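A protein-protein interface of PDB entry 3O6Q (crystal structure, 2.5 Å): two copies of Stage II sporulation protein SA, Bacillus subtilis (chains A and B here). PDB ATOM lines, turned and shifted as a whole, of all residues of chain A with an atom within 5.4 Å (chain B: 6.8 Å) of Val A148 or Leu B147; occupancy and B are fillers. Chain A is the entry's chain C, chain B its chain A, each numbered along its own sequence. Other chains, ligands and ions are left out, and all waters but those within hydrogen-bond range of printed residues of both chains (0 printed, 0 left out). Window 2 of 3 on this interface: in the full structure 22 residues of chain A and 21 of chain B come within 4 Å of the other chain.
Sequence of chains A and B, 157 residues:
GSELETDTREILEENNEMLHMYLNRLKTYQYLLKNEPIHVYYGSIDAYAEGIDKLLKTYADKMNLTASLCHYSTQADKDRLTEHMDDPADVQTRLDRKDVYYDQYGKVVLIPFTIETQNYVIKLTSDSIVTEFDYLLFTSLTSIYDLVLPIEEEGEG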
ATOM      1  N   LEU A  33      13.119 -34.922 -28.938  1.00  0.00           N
ATOM      2  CA  LEU A  33      14.138 -33.901 -28.744  1.00  0.00           C
ATOM      3  C   LEU A  33      13.458 -32.524 -28.772  1.00  0.00           C
ATOM      4  O   LEU A  33      13.847 -31.615 -28.061  1.00  0.00           O
ATOM      5  CB  LEU A  33      15.264 -34.005 -29.816  1.00  0.00           C
ATOM      6  CG  LEU A  33      16.314 -35.103 -29.528  1.00  0.00           C
ATOM      7  CD1 LEU A  33      17.299 -35.409 -30.670  1.00  0.00           C
ATOM      8  CD2 LEU A  33      17.034 -34.775 -28.227  1.00  0.00           C
ATOM      9  N   ILE A  38      13.997 -32.649 -21.041  1.00  0.00           N
ATOM     10  CA  ILE A  38      14.993 -33.540 -20.489  1.00  0.00           C
ATOM     11  C   ILE A  38      15.172 -33.207 -19.017  1.00  0.00           C
ATOM     12  O   ILE A  38      15.403 -32.063 -18.665  1.00  0.00           O
ATOM     13  CB  ILE A  38      16.306 -33.466 -21.273  1.00  0.00           C
ATOM     14  CG1 ILE A  38      16.014 -33.812 -22.752  1.00  0.00           C
ATOM     15  CG2 ILE A  38      17.318 -34.409 -20.699  1.00  0.00           C
ATOM     16  CD1 ILE A  38      17.193 -34.057 -23.631  1.00  0.00           C
ATOM     17  N   VAL A  40      17.535 -33.561 -16.052  1.00  0.00           N
ATOM     18  CA  VAL A  40      18.972 -33.800 -15.920  1.00  0.00           C
ATOM     19  C   VAL A  40      19.324 -34.134 -14.499  1.00  0.00           C
ATOM     20  O   VAL A  40      19.180 -33.298 -13.609  1.00  0.00           O
ATOM     21  CB  VAL A  40      19.807 -32.599 -16.403  1.00  0.00           C
ATOM     22  CG1 VAL A  40      21.275 -32.924 -16.295  1.00  0.00           C
ATOM     23  CG2 VAL A  40      19.446 -32.244 -17.836  1.00  0.00           C
ATOM     24  N   SER A 143      24.952 -39.275 -25.870  1.00  0.00           N
ATOM     25  CA  SER A 143      25.791 -38.132 -26.170  1.00  0.00           C
ATOM     26  C   SER A 143      25.086 -36.804 -25.897  1.00  0.00           C
ATOM     27  O   SER A 143      25.681 -35.892 -25.367  1.00  0.00           O
ATOM     28  CB  SER A 143      26.331 -38.211 -27.609  1.00  0.00           C
ATOM     29  OG  SER A 143      27.225 -39.347 -27.749  1.00  0.00           O
ATOM     30  N   ILE A 144      23.822 -36.682 -26.286  1.00  0.00           N
ATOM     31  CA  ILE A 144      23.062 -35.474 -26.021  1.00  0.00           C
ATOM     32  C   ILE A 144      22.964 -35.264 -24.519  1.00  0.00           C
ATOM     33  O   ILE A 144      23.078 -34.146 -24.027  1.00  0.00           O
ATOM     34  CB  ILE A 144      21.652 -35.526 -26.669  1.00  0.00           C
ATOM     35  CG1 ILE A 144      21.787 -35.572 -28.219  1.00  0.00           C
ATOM     36  CG2 ILE A 144      20.793 -34.337 -26.216  1.00  0.00           C
ATOM     37  CD1 ILE A 144      20.634 -36.394 -29.011  1.00  0.00           C
ATOM     38  N   TYR A 145      22.736 -36.331 -23.776  1.00  0.00           N
ATOM     39  CA  TYR A 145      22.640 -36.170 -22.332  1.00  0.00           C
ATOM     40  C   TYR A 145      23.924 -35.523 -21.805  1.00  0.00           C
ATOM     41  O   TYR A 145      23.873 -34.571 -21.035  1.00  0.00           O
ATOM     42  CB  TYR A 145      22.363 -37.497 -21.661  1.00  0.00           C
ATOM     43  CG  TYR A 145      21.994 -37.380 -20.175  1.00  0.00           C
ATOM     44  CD1 TYR A 145      20.675 -37.200 -19.745  1.00  0.00           C
ATOM     45  CD2 TYR A 145      22.973 -37.499 -19.201  1.00  0.00           C
ATOM     46  CE1 TYR A 145      20.348 -37.102 -18.332  1.00  0.00           C
ATOM     47  CE2 TYR A 145      22.655 -37.418 -17.820  1.00  0.00           C
ATOM     48  CZ  TYR A 145      21.354 -37.211 -17.400  1.00  0.00           C
ATOM     49  OH  TYR A 145      21.092 -37.161 -16.046  1.00  0.00           O
ATOM     50  N   ASP A 146      25.071 -36.030 -22.241  1.00  0.00           N
ATOM     51  CA  ASP A 146      26.354 -35.527 -21.750  1.00  0.00           C
ATOM     52  C   ASP A 146      26.511 -34.064 -22.115  1.00  0.00           C
ATOM     53  O   ASP A 146      26.952 -33.253 -21.310  1.00  0.00           O
ATOM     54  CB  ASP A 146      27.462 -36.361 -22.369  1.00  0.00           C
ATOM     55  CG  ASP A 146      28.817 -36.139 -21.772  1.00  0.00           C
ATOM     56  OD1 ASP A 146      29.092 -35.116 -21.084  1.00  0.00           O
ATOM     57  OD2 ASP A 146      29.661 -37.002 -22.101  1.00  0.00           O
ATOM     58  N   LEU A 147      26.128 -33.711 -23.332  1.00  0.00           N
ATOM     59  CA  LEU A 147      26.287 -32.325 -23.808  1.00  0.00           C
ATOM     60  C   LEU A 147      25.406 -31.318 -23.077  1.00  0.00           C
ATOM     61  O   LEU A 147      25.709 -30.157 -23.038  1.00  0.00           O
ATOM     62  CB  LEU A 147      25.999 -32.253 -25.305  1.00  0.00           C
ATOM     63  CG  LEU A 147      27.069 -32.873 -26.220  1.00  0.00           C
ATOM     64  CD1 LEU A 147      26.494 -33.062 -27.624  1.00  0.00           C
ATOM     65  CD2 LEU A 147      28.390 -32.025 -26.223  1.00  0.00           C
ATOM     66  N   VAL A 148      24.312 -31.788 -22.505  1.00  0.00           N
ATOM     67  CA  VAL A 148      23.331 -30.949 -21.821  1.00  0.00           C
ATOM     68  C   VAL A 148      23.682 -30.733 -20.342  1.00  0.00           C
ATOM     69  O   VAL A 148      23.091 -29.870 -19.681  1.00  0.00           O
ATOM     70  CB  VAL A 148      21.913 -31.584 -22.014  1.00  0.00           C
ATOM     71  CG1 VAL A 148      21.032 -31.402 -20.814  1.00  0.00           C
ATOM     72  CG2 VAL A 148      21.256 -31.088 -23.331  1.00  0.00           C
ATOM     73  N   LEU A 149      24.673 -31.455 -19.828  1.00  0.00           N
ATOM     74  CA  LEU A 149      25.158 -31.203 -18.458  1.00  0.00           C
ATOM     75  C   LEU A 149      25.853 -29.853 -18.272  1.00  0.00           C
ATOM     76  O   LEU A 149      26.471 -29.346 -19.204  1.00  0.00           O
ATOM     77  CB  LEU A 149      26.152 -32.280 -18.049  1.00  0.00           C
ATOM     78  CG  LEU A 149      25.581 -33.673 -17.825  1.00  0.00           C
ATOM     79  CD1 LEU A 149      26.672 -34.627 -17.322  1.00  0.00           C
ATOM     80  CD2 LEU A 149      24.420 -33.656 -16.867  1.00  0.00           C
ATOM     81  N   PRO A 150      25.807 -29.291 -17.048  1.00  0.00           N
ATOM     82  CA  PRO A 150      26.520 -28.056 -16.727  1.00  0.00           C
ATOM     83  C   PRO A 150      27.846 -28.310 -16.023  1.00  0.00           C
ATOM     84  O   PRO A 150      28.545 -29.251 -16.382  1.00  0.00           O
ATOM     85  CB  PRO A 150      25.562 -27.377 -15.769  1.00  0.00           C
ATOM     86  CG  PRO A 150      25.027 -28.545 -14.968  1.00  0.00           C
ATOM     87  CD  PRO A 150      24.999 -29.739 -15.899  1.00  0.00           C
ATOM     88  N   TYR B  48      22.379 -16.514 -32.019  1.00  0.00           N
ATOM     89  CA  TYR B  48      21.659 -17.768 -32.067  1.00  0.00           C
ATOM     90  C   TYR B  48      21.575 -18.259 -33.508  1.00  0.00           C
ATOM     91  O   TYR B  48      21.871 -19.409 -33.780  1.00  0.00           O
ATOM     92  CB  TYR B  48      20.248 -17.602 -31.475  1.00  0.00           C
ATOM     93  CG  TYR B  48      19.577 -18.903 -31.070  1.00  0.00           C
ATOM     94  CD1 TYR B  48      19.518 -19.292 -29.730  1.00  0.00           C
ATOM     95  CD2 TYR B  48      19.030 -19.754 -32.013  1.00  0.00           C
ATOM     96  CE1 TYR B  48      18.910 -20.507 -29.324  1.00  0.00           C
ATOM     97  CE2 TYR B  48      18.431 -20.963 -31.623  1.00  0.00           C
ATOM     98  CZ  TYR B  48      18.369 -21.329 -30.270  1.00  0.00           C
ATOM     99  OH  TYR B  48      17.765 -22.523 -29.866  1.00  0.00           O
ATOM    100  N   SER B 140      16.305 -32.143 -35.516  1.00  0.00           N
ATOM    101  CA  SER B 140      16.904 -32.684 -34.292  1.00  0.00           C
ATOM    102  C   SER B 140      18.059 -31.870 -33.796  1.00  0.00           C
ATOM    103  O   SER B 140      18.186 -31.619 -32.606  1.00  0.00           O
ATOM    104  CB  SER B 140      17.420 -34.097 -34.540  1.00  0.00           C
ATOM    105  OG  SER B 140      16.296 -34.959 -34.730  1.00  0.00           O
ATOM    106  N   THR B 142      18.793 -28.634 -34.364  1.00  0.00           N
ATOM    107  CA  THR B 142      18.280 -27.367 -33.844  1.00  0.00           C
ATOM    108  C   THR B 142      17.740 -27.568 -32.442  1.00  0.00           C
ATOM    109  O   THR B 142      17.890 -26.696 -31.606  1.00  0.00           O
ATOM    110  CB  THR B 142      17.143 -26.788 -34.730  1.00  0.00           C
ATOM    111  OG1 THR B 142      16.022 -27.672 -34.720  1.00  0.00           O
ATOM    112  CG2 THR B 142      17.591 -26.574 -36.173  1.00  0.00           C
ATOM    113  N   SER B 143      17.132 -28.712 -32.165  1.00  0.00           N
ATOM    114  CA  SER B 143      16.646 -29.002 -30.807  1.00  0.00           C
ATOM    115  C   SER B 143      17.780 -29.230 -29.839  1.00  0.00           C
ATOM    116  O   SER B 143      17.760 -28.687 -28.737  1.00  0.00           O
ATOM    117  CB  SER B 143      15.668 -30.184 -30.800  1.00  0.00           C
ATOM    118  OG  SER B 143      14.475 -29.820 -31.492  1.00  0.00           O
ATOM    119  N   ILE B 144      18.797 -29.973 -30.259  1.00  0.00           N
ATOM    120  CA  ILE B 144      19.978 -30.156 -29.440  1.00  0.00           C
ATOM    121  C   ILE B 144      20.659 -28.830 -29.165  1.00  0.00           C
ATOM    122  O   ILE B 144      21.089 -28.573 -28.060  1.00  0.00           O
ATOM    123  CB  ILE B 144      20.976 -31.094 -30.105  1.00  0.00           C
ATOM    124  CG1 ILE B 144      20.358 -32.504 -30.230  1.00  0.00           C
ATOM    125  CG2 ILE B 144      22.296 -31.110 -29.313  1.00  0.00           C
ATOM    126  CD1 ILE B 144      20.907 -33.318 -31.394  1.00  0.00           C
ATOM    127  N   TYR B 145      20.723 -27.956 -30.153  1.00  0.00           N
ATOM    128  CA  TYR B 145      21.293 -26.623 -29.927  1.00  0.00           C
ATOM    129  C   TYR B 145      20.594 -25.892 -28.801  1.00  0.00           C
ATOM    130  O   TYR B 145      21.248 -25.365 -27.884  1.00  0.00           O
ATOM    131  CB  TYR B 145      21.250 -25.787 -31.198  1.00  0.00           C
ATOM    132  CG  TYR B 145      22.045 -24.500 -31.151  1.00  0.00           C
ATOM    133  CD1 TYR B 145      23.404 -24.481 -31.469  1.00  0.00           C
ATOM    134  CD2 TYR B 145      21.434 -23.287 -30.831  1.00  0.00           C
ATOM    135  CE1 TYR B 145      24.127 -23.298 -31.458  1.00  0.00           C
ATOM    136  CE2 TYR B 145      22.150 -22.112 -30.835  1.00  0.00           C
ATOM    137  CZ  TYR B 145      23.498 -22.139 -31.147  1.00  0.00           C
ATOM    138  OH  TYR B 145      24.188 -20.965 -31.073  1.00  0.00           O
ATOM    139  N   ASP B 146      19.265 -25.887 -28.829  1.00  0.00           N
ATOM    140  CA  ASP B 146      18.506 -25.162 -27.800  1.00  0.00           C
ATOM    141  C   ASP B 146      18.745 -25.771 -26.424  1.00  0.00           C
ATOM    142  O   ASP B 146      18.915 -25.053 -25.435  1.00  0.00           O
ATOM    143  CB  ASP B 146      17.038 -25.216 -28.109  1.00  0.00           C
ATOM    144  CG  ASP B 146      16.247 -24.204 -27.294  1.00  0.00           C
ATOM    145  OD1 ASP B 146      16.273 -24.264 -26.039  1.00  0.00           O
ATOM    146  OD2 ASP B 146      15.602 -23.319 -27.900  1.00  0.00           O
ATOM    147  N   LEU B 147      18.785 -27.101 -26.372  1.00  0.00           N
ATOM    148  CA  LEU B 147      18.947 -27.808 -25.100  1.00  0.00           C
ATOM    149  C   LEU B 147      20.316 -27.610 -24.468  1.00  0.00           C
ATOM    150  O   LEU B 147      20.459 -27.753 -23.272  1.00  0.00           O
ATOM    151  CB  LEU B 147      18.722 -29.300 -25.289  1.00  0.00           C
ATOM    152  CG  LEU B 147      17.261 -29.656 -25.518  1.00  0.00           C
ATOM    153  CD1 LEU B 147      17.178 -31.082 -26.065  1.00  0.00           C
ATOM    154  CD2 LEU B 147      16.457 -29.462 -24.242  1.00  0.00           C
ATOM    155  N   VAL B 148      21.308 -27.293 -25.281  1.00  0.00           N
ATOM    156  CA  VAL B 148      22.642 -27.110 -24.814  1.00  0.00           C
ATOM    157  C   VAL B 148      22.854 -25.696 -24.235  1.00  0.00           C
ATOM    158  O   VAL B 148      23.813 -25.477 -23.498  1.00  0.00           O
ATOM    159  CB  VAL B 148      23.625 -27.428 -25.929  1.00  0.00           C
ATOM    160  CG1 VAL B 148      24.872 -26.622 -25.767  1.00  0.00           C
ATOM    161  CG2 VAL B 148      23.915 -28.931 -25.940  1.00  0.00           C
ATOM    162  N   LEU B 149      21.947 -24.755 -24.504  1.00  0.00           N
ATOM    163  CA  LEU B 149      22.061 -23.403 -23.916  1.00  0.00           C
ATOM    164  C   LEU B 149      21.908 -23.373 -22.385  1.00  0.00           C
ATOM    165  O   LEU B 149      21.119 -24.140 -21.827  1.00  0.00           O
ATOM    166  CB  LEU B 149      21.017 -22.471 -24.511  1.00  0.00           C
ATOM    167  CG  LEU B 149      21.209 -22.107 -25.959  1.00  0.00           C
ATOM    168  CD1 LEU B 149      20.208 -21.035 -26.298  1.00  0.00           C
ATOM    169  CD2 LEU B 149      22.624 -21.601 -26.132  1.00  0.00           C
ATOM    170  N   PRO B 150      22.652 -22.485 -21.704  1.00  0.00           N
ATOM    171  CA  PRO B 150      22.479 -22.382 -20.247  1.00  0.00           C
ATOM    172  C   PRO B 150      21.199 -21.632 -19.883  1.00  0.00           C
ATOM    173  O   PRO B 150      20.193 -22.255 -19.571  1.00  0.00           O
ATOM    174  CB  PRO B 150      23.721 -21.592 -19.789  1.00  0.00           C
ATOM    175  CG  PRO B 150      24.669 -21.593 -20.975  1.00  0.00           C
ATOM    176  CD  PRO B 150      23.787 -21.671 -22.180  1.00  0.00           C
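Ser B143 touches Leu A33. O of Leu A33 touches CD1 of Leu B147 (3.9 Å). Ile A38 touches Leu B147 (CD1 to CD1, 3.8 Å). Ile A144 touches Ile B144 (CD1 to CD1, 3.9 Å). Leu A147 touches Val B148 (O to CG2, 3.6 Å). O of Leu B147 touches CG2 of Val A148, 3.4 Å away.
Val A148 touches just one residue of chain B: Leu B147. Printed residues of chain A within 4 Å of Leu B147: Leu A33 (3.9 Å), Ile A38 (3.8 Å) and Val A148 (3.4 Å). Printed residues of chain B within 4 Å of Leu A147: Val B148. Printed residues of chain B within 4 Å of Leu A33: Ser B143 and Leu B147. Of the printed residues of chain A, Ile B144 touches Ile A144. Of the printed residues of chain B, Ile A144 touches Ile B144.
Of the 11 printed residues of chain B, 4 touch a printed residue of chain A. Printed residues of chain B that touch a printed residue of chain A: Ser B143, Ile B144, Leu B147 and Val B148. Hydrophobic or aromatic side chains of chain B that line the printed part of chain A: Ile B144, Leu B147 and Val B148. Of the 11 printed residues of chain A, 5 touch a printed residue of chain B. Printed residues of chain A that touch a printed residue of chain B: Leu A33, Ile A38, Ile A144, Leu A147 and Val A148. Among the printed residues, no Asp or Glu carboxylate lies within 4 Å of a Lys or Arg side-chain nitrogen of the other chain.
Ile B144 touches its own counterpart, Ile A144. Leu A147 touches Val B148, and with the chains exchanged Val A148 touches Leu B147. Of the 6 pairs that touch across the chains among the printed residues, 3 have their exchanged pair printed and touching as well.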
